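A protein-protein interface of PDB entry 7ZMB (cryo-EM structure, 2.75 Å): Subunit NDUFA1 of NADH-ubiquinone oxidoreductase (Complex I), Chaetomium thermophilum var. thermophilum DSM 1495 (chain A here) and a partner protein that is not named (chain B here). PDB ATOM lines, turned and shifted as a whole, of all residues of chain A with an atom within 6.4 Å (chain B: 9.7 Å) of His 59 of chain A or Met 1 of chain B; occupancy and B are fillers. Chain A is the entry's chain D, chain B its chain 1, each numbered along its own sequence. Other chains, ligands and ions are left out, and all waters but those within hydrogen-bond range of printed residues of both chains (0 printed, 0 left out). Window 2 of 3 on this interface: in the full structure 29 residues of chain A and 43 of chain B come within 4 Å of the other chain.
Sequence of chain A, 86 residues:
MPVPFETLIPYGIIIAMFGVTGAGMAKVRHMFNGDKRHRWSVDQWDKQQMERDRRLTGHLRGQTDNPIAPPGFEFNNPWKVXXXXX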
ATOM      1  N   MET A  31     -34.605  -9.382 -10.597  1.00  0.00           N
ATOM      2  CA  MET A  31     -33.721  -8.220 -10.647  1.00  0.00           C
ATOM      3  C   MET A  31     -32.355  -8.576 -11.214  1.00  0.00           C
ATOM      4  O   MET A  31     -31.808  -7.839 -12.040  1.00  0.00           O
ATOM      5  CB  MET A  31     -33.561  -7.626  -9.249  1.00  0.00           C
ATOM      6  CG  MET A  31     -32.752  -6.347  -9.208  1.00  0.00           C
ATOM      7  SD  MET A  31     -33.526  -4.995 -10.115  1.00  0.00           S
ATOM      8  CE  MET A  31     -34.886  -4.591  -9.023  1.00  0.00           C
ATOM      9  N   PHE A  32     -31.761  -9.682 -10.779  1.00  0.00           N
ATOM     10  CA  PHE A  32     -30.381 -10.036 -11.211  1.00  0.00           C
ATOM     11  C   PHE A  32     -30.316 -10.379 -12.706  1.00  0.00           C
ATOM     12  O   PHE A  32     -29.242 -10.215 -13.303  1.00  0.00           O
ATOM     13  CB  PHE A  32     -29.934 -11.267 -10.431  1.00  0.00           C
ATOM     14  CG  PHE A  32     -28.446 -11.429 -10.284  1.00  0.00           C
ATOM     15  CD1 PHE A  32     -27.650 -10.347  -9.954  1.00  0.00           C
ATOM     16  CD2 PHE A  32     -27.848 -12.665 -10.460  1.00  0.00           C
ATOM     17  CE1 PHE A  32     -26.283 -10.493  -9.805  1.00  0.00           C
ATOM     18  CE2 PHE A  32     -26.479 -12.810 -10.309  1.00  0.00           C
ATOM     19  CZ  PHE A  32     -25.703 -11.724  -9.982  1.00  0.00           C
ATOM     20  N   ASN A  33     -31.419 -10.828 -13.306  1.00  0.00           N
ATOM     21  CA  ASN A  33     -31.398 -11.315 -14.709  1.00  0.00           C
ATOM     22  C   ASN A  33     -31.873 -10.223 -15.659  1.00  0.00           C
ATOM     23  O   ASN A  33     -32.000 -10.516 -16.857  1.00  0.00           O
ATOM     24  CB  ASN A  33     -32.096 -12.669 -14.836  1.00  0.00           C
ATOM     25  CG  ASN A  33     -31.274 -13.809 -14.271  1.00  0.00           C
ATOM     26  OD1 ASN A  33     -30.482 -14.416 -14.984  1.00  0.00           O
ATOM     27  ND2 ASN A  33     -31.444 -14.101 -12.993  1.00  0.00           N
ATOM     28  N   GLY A  34     -32.105  -9.021 -15.157  1.00  0.00           N
ATOM     29  CA  GLY A  34     -32.442  -7.876 -16.017  1.00  0.00           C
ATOM     30  C   GLY A  34     -33.934  -7.734 -16.138  1.00  0.00           C
ATOM     31  O   GLY A  34     -34.422  -7.666 -17.277  1.00  0.00           O
ATOM     32  N   LYS A  36     -36.029  -9.892 -15.698  1.00  0.00           N
ATOM     33  CA  LYS A  36     -36.412 -11.046 -16.493  1.00  0.00           C
ATOM     34  C   LYS A  36     -36.391 -12.281 -15.611  1.00  0.00           C
ATOM     35  O   LYS A  36     -35.612 -12.366 -14.660  1.00  0.00           O
ATOM     36  CB  LYS A  36     -35.470 -11.247 -17.685  1.00  0.00           C
ATOM     37  CG  LYS A  36     -35.571 -10.175 -18.752  1.00  0.00           C
ATOM     38  CD  LYS A  36     -34.348 -10.190 -19.654  1.00  0.00           C
ATOM     39  CE  LYS A  36     -34.659  -9.631 -21.029  1.00  0.00           C
ATOM     40  NZ  LYS A  36     -35.818 -10.320 -21.658  1.00  0.00           N
ATOM     41  N   MET A  50     -25.958 -18.662 -23.375  1.00  0.00           N
ATOM     42  CA  MET A  50     -25.951 -17.451 -22.503  1.00  0.00           C
ATOM     43  C   MET A  50     -24.662 -16.660 -22.710  1.00  0.00           C
ATOM     44  O   MET A  50     -24.702 -15.427 -22.638  1.00  0.00           O
ATOM     45  CB  MET A  50     -26.150 -17.772 -21.016  1.00  0.00           C
ATOM     46  CG  MET A  50     -27.611 -17.911 -20.649  1.00  0.00           C
ATOM     47  SD  MET A  50     -27.918 -18.366 -18.932  1.00  0.00           S
ATOM     48  CE  MET A  50     -27.325 -20.055 -18.927  1.00  0.00           C
ATOM     49  N   ASP A  53     -24.826 -14.700 -25.750  1.00  0.00           N
ATOM     50  CA  ASP A  53     -25.730 -13.524 -25.640  1.00  0.00           C
ATOM     51  C   ASP A  53     -24.886 -12.376 -25.097  1.00  0.00           C
ATOM     52  O   ASP A  53     -25.073 -11.246 -25.553  1.00  0.00           O
ATOM     53  CB  ASP A  53     -26.941 -13.827 -24.757  1.00  0.00           C
ATOM     54  CG  ASP A  53     -27.945 -14.763 -25.404  1.00  0.00           C
ATOM     55  OD1 ASP A  53     -27.693 -15.199 -26.539  1.00  0.00           O
ATOM     56  OD2 ASP A  53     -28.970 -15.044 -24.762  1.00  0.00           O
ATOM     57  N   ARG A  54     -23.985 -12.679 -24.166  1.00  0.00           N
ATOM     58  CA  ARG A  54     -23.019 -11.669 -23.662  1.00  0.00           C
ATOM     59  C   ARG A  54     -22.155 -11.187 -24.826  1.00  0.00           C
ATOM     60  O   ARG A  54     -21.862  -9.993 -24.871  1.00  0.00           O
ATOM     61  CB  ARG A  54     -22.185 -12.282 -22.542  1.00  0.00           C
ATOM     62  CG  ARG A  54     -21.459 -11.268 -21.674  1.00  0.00           C
ATOM     63  CD  ARG A  54     -20.265 -11.902 -20.994  1.00  0.00           C
ATOM     64  NE  ARG A  54     -20.548 -12.473 -19.688  1.00  0.00           N
ATOM     65  CZ  ARG A  54     -19.758 -13.339 -19.074  1.00  0.00           C
ATOM     66  NH1 ARG A  54     -20.075 -13.797 -17.877  1.00  0.00           N
ATOM     67  NH2 ARG A  54     -18.655 -13.755 -19.669  1.00  0.00           N
ATOM     68  N   ARG A  55     -21.777 -12.083 -25.735  1.00  0.00           N
ATOM     69  CA  ARG A  55     -20.962 -11.709 -26.913  1.00  0.00           C
ATOM     70  C   ARG A  55     -21.694 -10.695 -27.802  1.00  0.00           C
ATOM     71  O   ARG A  55     -21.006  -9.900 -28.451  1.00  0.00           O
ATOM     72  CB  ARG A  55     -20.520 -12.954 -27.679  1.00  0.00           C
ATOM     73  CG  ARG A  55     -19.499 -13.817 -26.958  1.00  0.00           C
ATOM     74  CD  ARG A  55     -19.311 -15.057 -27.800  1.00  0.00           C
ATOM     75  NE  ARG A  55     -18.804 -14.702 -29.112  1.00  0.00           N
ATOM     76  CZ  ARG A  55     -18.810 -15.508 -30.161  1.00  0.00           C
ATOM     77  NH1 ARG A  55     -19.311 -16.726 -30.054  1.00  0.00           N
ATOM     78  NH2 ARG A  55     -18.318 -15.094 -31.313  1.00  0.00           N
ATOM     79  N   LEU A  56     -23.027 -10.728 -27.830  1.00  0.00           N
ATOM     80  CA  LEU A  56     -23.813  -9.802 -28.686  1.00  0.00           C
ATOM     81  C   LEU A  56     -24.405  -8.633 -27.886  1.00  0.00           C
ATOM     82  O   LEU A  56     -24.722  -7.627 -28.517  1.00  0.00           O
ATOM     83  CB  LEU A  56     -24.919 -10.605 -29.371  1.00  0.00           C
ATOM     84  CG  LEU A  56     -24.478 -11.706 -30.329  1.00  0.00           C
ATOM     85  CD1 LEU A  56     -25.428 -12.891 -30.282  1.00  0.00           C
ATOM     86  CD2 LEU A  56     -24.373 -11.174 -31.744  1.00  0.00           C
ATOM     87  N   THR A  57     -24.580  -8.759 -26.563  1.00  0.00           N
ATOM     88  CA  THR A  57     -25.257  -7.705 -25.820  1.00  0.00           C
ATOM     89  C   THR A  57     -24.531  -7.243 -24.570  1.00  0.00           C
ATOM     90  O   THR A  57     -24.929  -6.222 -24.004  1.00  0.00           O
ATOM     91  CB  THR A  57     -26.673  -8.147 -25.410  1.00  0.00           C
ATOM     92  OG1 THR A  57     -26.592  -9.087 -24.335  1.00  0.00           O
ATOM     93  CG2 THR A  57     -27.413  -8.778 -26.570  1.00  0.00           C
ATOM     94  N   GLY A  58     -23.495  -7.945 -24.120  1.00  0.00           N
ATOM     95  CA  GLY A  58     -22.806  -7.616 -22.895  1.00  0.00           C
ATOM     96  C   GLY A  58     -23.455  -8.187 -21.653  1.00  0.00           C
ATOM     97  O   GLY A  58     -22.780  -8.390 -20.643  1.00  0.00           O
ATOM     98  N   HIS A  59     -24.749  -8.450 -21.711  1.00  0.00           N
ATOM     99  CA  HIS A  59     -25.485  -9.088 -20.636  1.00  0.00           C
ATOM    100  C   HIS A  59     -25.668 -10.552 -20.990  1.00  0.00           C
ATOM    101  O   HIS A  59     -26.009 -10.874 -22.131  1.00  0.00           O
ATOM    102  CB  HIS A  59     -26.840  -8.415 -20.440  1.00  0.00           C
ATOM    103  CG  HIS A  59     -27.528  -8.786 -19.165  1.00  0.00           C
ATOM    104  ND1 HIS A  59     -28.746  -9.424 -19.133  1.00  0.00           N
ATOM    105  CD2 HIS A  59     -27.167  -8.600 -17.874  1.00  0.00           C
ATOM    106  CE1 HIS A  59     -29.100  -9.626 -17.878  1.00  0.00           C
ATOM    107  NE2 HIS A  59     -28.162  -9.132 -17.095  1.00  0.00           N
ATOM    108  N   LEU A  60     -25.426 -11.452 -20.032  1.00  0.00           N
ATOM    109  CA  LEU A  60     -25.536 -12.916 -20.298  1.00  0.00           C
ATOM    110  C   LEU A  60     -26.971 -13.237 -20.699  1.00  0.00           C
ATOM    111  O   LEU A  60     -27.174 -14.247 -21.362  1.00  0.00           O
ATOM    112  CB  LEU A  60     -25.182 -13.702 -19.035  1.00  0.00           C
ATOM    113  CG  LEU A  60     -23.701 -13.934 -18.768  1.00  0.00           C
ATOM    114  CD1 LEU A  60     -23.466 -14.136 -17.280  1.00  0.00           C
ATOM    115  CD2 LEU A  60     -23.204 -15.129 -19.560  1.00  0.00           C
ATOM    116  N   ARG A  61     -27.921 -12.397 -20.303  1.00  0.00           N
ATOM    117  CA  ARG A  61     -29.356 -12.681 -20.530  1.00  0.00           C
ATOM    118  C   ARG A  61     -29.989 -11.643 -21.464  1.00  0.00           C
ATOM    119  O   ARG A  61     -31.216 -11.498 -21.412  1.00  0.00           O
ATOM    120  CB  ARG A  61     -30.011 -12.752 -19.151  1.00  0.00           C
ATOM    121  CG  ARG A  61     -29.687 -14.006 -18.354  1.00  0.00           C
ATOM    122  CD  ARG A  61     -30.424 -15.213 -18.896  1.00  0.00           C
ATOM    123  NE  ARG A  61     -31.772 -14.908 -19.351  1.00  0.00           N
ATOM    124  CZ  ARG A  61     -32.848 -14.912 -18.577  1.00  0.00           C
ATOM    125  NH1 ARG A  61     -34.032 -14.622 -19.085  1.00  0.00           N
ATOM    126  NH2 ARG A  61     -32.736 -15.201 -17.294  1.00  0.00           N
ATOM    127  N   GLY A  62     -29.185 -10.923 -22.253  1.00  0.00           N
ATOM    128  CA  GLY A  62     -29.703  -9.912 -23.202  1.00  0.00           C
ATOM    129  C   GLY A  62     -29.986 -10.509 -24.567  1.00  0.00           C
ATOM    130  O   GLY A  62     -29.207 -11.376 -24.983  1.00  0.00           O
ATOM    131  N   GLN A  63     -31.021 -10.040 -25.263  1.00  0.00           N
ATOM    132  CA  GLN A  63     -31.409 -10.707 -26.531  1.00  0.00           C
ATOM    133  C   GLN A  63     -31.485  -9.742 -27.713  1.00  0.00           C
ATOM    134  O   GLN A  63     -31.999  -8.641 -27.535  1.00  0.00           O
ATOM    135  CB  GLN A  63     -32.710 -11.495 -26.353  1.00  0.00           C
ATOM    136  CG  GLN A  63     -32.749 -12.391 -25.123  1.00  0.00           C
ATOM    137  CD  GLN A  63     -32.010 -13.694 -25.288  1.00  0.00           C
ATOM    138  OE1 GLN A  63     -31.757 -14.157 -26.395  1.00  0.00           O
ATOM    139  NE2 GLN A  63     -31.670 -14.311 -24.168  1.00  0.00           N
ATOM    140  N   MET B   1     -24.576  -9.977 -15.553  1.00  0.00           N
ATOM    141  CA  MET B   1     -25.696  -9.786 -14.593  1.00  0.00           C
ATOM    142  C   MET B   1     -25.859  -8.300 -14.258  1.00  0.00           C
ATOM    143  O   MET B   1     -25.154  -7.492 -14.882  1.00  0.00           O
ATOM    144  CB  MET B   1     -25.493 -10.628 -13.338  1.00  0.00           C
ATOM    145  CG  MET B   1     -25.401 -12.117 -13.640  1.00  0.00           C
ATOM    146  SD  MET B   1     -26.778 -12.750 -14.628  1.00  0.00           S
ATOM    147  CE  MET B   1     -26.474 -14.512 -14.539  1.00  0.00           C
ATOM    148  N   SER B   2     -26.771  -7.935 -13.356  1.00  0.00           N
ATOM    149  CA  SER B   2     -27.059  -6.489 -13.140  1.00  0.00           C
ATOM    150  C   SER B   2     -26.311  -5.936 -11.927  1.00  0.00           C
ATOM    151  O   SER B   2     -25.670  -4.877 -12.051  1.00  0.00           O
ATOM    152  CB  SER B   2     -28.547  -6.261 -13.052  1.00  0.00           C
ATOM    153  OG  SER B   2     -29.241  -7.023 -14.029  1.00  0.00           O
ATOM    154  N   TYR B   3     -26.351  -6.643 -10.809  1.00  0.00           N
ATOM    155  CA  TYR B   3     -25.543  -6.219  -9.648  1.00  0.00           C
ATOM    156  C   TYR B   3     -24.450  -7.251  -9.381  1.00  0.00           C
ATOM    157  O   TYR B   3     -24.230  -8.097 -10.247  1.00  0.00           O
ATOM    158  CB  TYR B   3     -26.408  -5.902  -8.428  1.00  0.00           C
ATOM    159  CG  TYR B   3     -27.390  -6.959  -7.991  1.00  0.00           C
ATOM    160  CD1 TYR B   3     -28.617  -7.105  -8.616  1.00  0.00           C
ATOM    161  CD2 TYR B   3     -27.115  -7.775  -6.909  1.00  0.00           C
ATOM    162  CE1 TYR B   3     -29.527  -8.060  -8.199  1.00  0.00           C
ATOM    163  CE2 TYR B   3     -28.017  -8.729  -6.477  1.00  0.00           C
ATOM    164  CZ  TYR B   3     -29.226  -8.878  -7.127  1.00  0.00           C
ATOM    165  OH  TYR B   3     -30.113  -9.823  -6.704  1.00  0.00           O
ATOM    166  N   SER B   4     -23.821  -7.182  -8.204  1.00  0.00           N
ATOM    167  CA  SER B   4     -22.701  -8.048  -7.868  1.00  0.00           C
ATOM    168  C   SER B   4     -23.136  -9.495  -7.671  1.00  0.00           C
ATOM    169  O   SER B   4     -24.240  -9.783  -7.209  1.00  0.00           O
ATOM    170  CB  SER B   4     -22.017  -7.540  -6.600  1.00  0.00           C
ATOM    171  OG  SER B   4     -21.149  -8.512  -6.067  1.00  0.00           O
ATOM    172  N   GLN B   5     -22.237 -10.411  -8.039  1.00  0.00           N
ATOM    173  CA  GLN B   5     -22.416 -11.822  -7.725  1.00  0.00           C
ATOM    174  C   GLN B   5     -22.482 -12.057  -6.225  1.00  0.00           C
ATOM    175  O   GLN B   5     -23.327 -12.822  -5.747  1.00  0.00           O
ATOM    176  CB  GLN B   5     -21.272 -12.639  -8.326  1.00  0.00           C
ATOM    177  CG  GLN B   5     -21.560 -14.119  -8.568  1.00  0.00           C
ATOM    178  CD  GLN B   5     -22.867 -14.393  -9.281  1.00  0.00           C
ATOM    179  OE1 GLN B   5     -23.394 -13.544  -9.995  1.00  0.00           O
ATOM    180  NE2 GLN B   5     -23.402 -15.592  -9.086  1.00  0.00           N
ATOM    181  N   THR B   6     -21.583 -11.434  -5.468  1.00  0.00           N
ATOM    182  CA  THR B   6     -21.517 -11.712  -4.040  1.00  0.00           C
ATOM    183  C   THR B   6     -22.753 -11.205  -3.315  1.00  0.00           C
ATOM    184  O   THR B   6     -23.222 -11.849  -2.370  1.00  0.00           O
ATOM    185  CB  THR B   6     -20.247 -11.106  -3.448  1.00  0.00           C
ATOM    186  OG1 THR B   6     -19.110 -11.683  -4.094  1.00  0.00           O
ATOM    187  CG2 THR B   6     -20.155 -11.391  -1.969  1.00  0.00           C
ATOM    188  N   ASN B   8     -25.853 -10.844  -4.663  1.00  0.00           N
ATOM    189  CA  ASN B   8     -26.963 -11.723  -5.014  1.00  0.00           C
ATOM    190  C   ASN B   8     -26.895 -13.009  -4.211  1.00  0.00           C
ATOM    191  O   ASN B   8     -27.895 -13.460  -3.651  1.00  0.00           O
ATOM    192  CB  ASN B   8     -26.942 -12.018  -6.516  1.00  0.00           C
ATOM    193  CG  ASN B   8     -27.971 -13.058  -6.929  1.00  0.00           C
ATOM    194  OD1 ASN B   8     -27.644 -14.225  -7.121  1.00  0.00           O
ATOM    195  ND2 ASN B   8     -29.215 -12.633  -7.080  1.00  0.00           N
ATOM    196  N   SER B   9     -25.703 -13.595  -4.122  1.00  0.00           N
ATOM    197  CA  SER B   9     -25.497 -14.767  -3.283  1.00  0.00           C
ATOM    198  C   SER B   9     -25.777 -14.463  -1.820  1.00  0.00           C
ATOM    199  O   SER B   9     -26.315 -15.306  -1.095  1.00  0.00           O
ATOM    200  CB  SER B   9     -24.068 -15.267  -3.462  1.00  0.00           C
ATOM    201  OG  SER B   9     -23.722 -16.159  -2.429  1.00  0.00           O
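The side-chain hydroxyl (OG) of Ser 2 of chain B lies within hydrogen-bond range of the backbone carbonyl oxygen (O) of Met 31 of chain A (3.3 Å). O of Phe 32 of chain A lies within hydrogen-bond range of OG of Ser 2 of chain B (3.3 Å). The backbone carbonyl oxygen of Phe 32 of chain A lies close to the side-chain sulfur of Met 1 of chain B.
ND2 of Asn 8 of chain B is in hydrogen-bond range of OH of Tyr 3 of chain B (3.0 Å). The side-chain hydroxyl of Ser 4 of chain B is in hydrogen-bond range of the backbone NH of Thr 6 of chain B (3.0 Å). The backbone NH of Arg 54 of chain A lies within hydrogen-bond range of the backbone carbonyl oxygen of His 59 of chain A. The side-chain hydroxyl of Thr 57 of chain A is in hydrogen-bond range of the backbone carbonyl oxygen of His 59 of chain A (2.9 Å). ND1 of His 59 of chain A sits close to N of Arg 61 of chain A (3.3 Å). A ring nitrogen (ND1) of His 59 of chain A is in hydrogen-bond range of the backbone NH (N) of Gly 62 of chain A (3.5 Å).
Among the printed residues, merely in contact across the chains: Phe 32 of chain A with Gln 5 of chain B (2.9 Å), Phe 32 of chain A with Tyr 3 of chain B (3.2 Å), Phe 32 of chain A with Ser 4 of chain B (3.4 Å), Phe 32 of chain A with Asn 8 of chain B (3.5 Å), His 59 of chain A with Met 1 of chain B (3.6 Å), Gly 34 of chain A with Ser 2 of chain B (3.7 Å), Met 31 of chain A with Tyr 3 of chain B (3.8 Å) and His 59 of chain A with Ser 2 of chain B (3.9 Å).
No residue of chain B comes within 4 Å of Asn 33 of chain A. Met 50 of chain A touches none of the printed residues of chain B. No residue of chain B comes within 4 Å of Gly 58 of chain A. His 59 of chain A touches two residues of chain B. No residue of chain B comes within 4 Å of Leu 60 of chain A. Of chain A, only Phe 32 and His 59 come within 4 Å of Met 1 of chain B. Printed residues of chain A within 4 Å of Ser 4 of chain B: Phe 32. Of the printed residues of chain A, Gln 5 of chain B touches Phe 32. Of the printed residues of chain A, Asn 8 of chain B touches Phe 32. The nearest residue of chain A that does not touch Met 1 of chain B is Asn 33 of chain A (4.03 Å).
Of the 8 printed residues of chain B, 6 touch a printed residue of chain A. Hydrophobic or aromatic side chains of chain B within 4 Å of the printed part of chain A: Met 1 and Tyr 3. Among the printed residues, no Asp or Glu carboxylate lies within 4 Å of a Lys or Arg side-chain nitrogen of the other chain.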
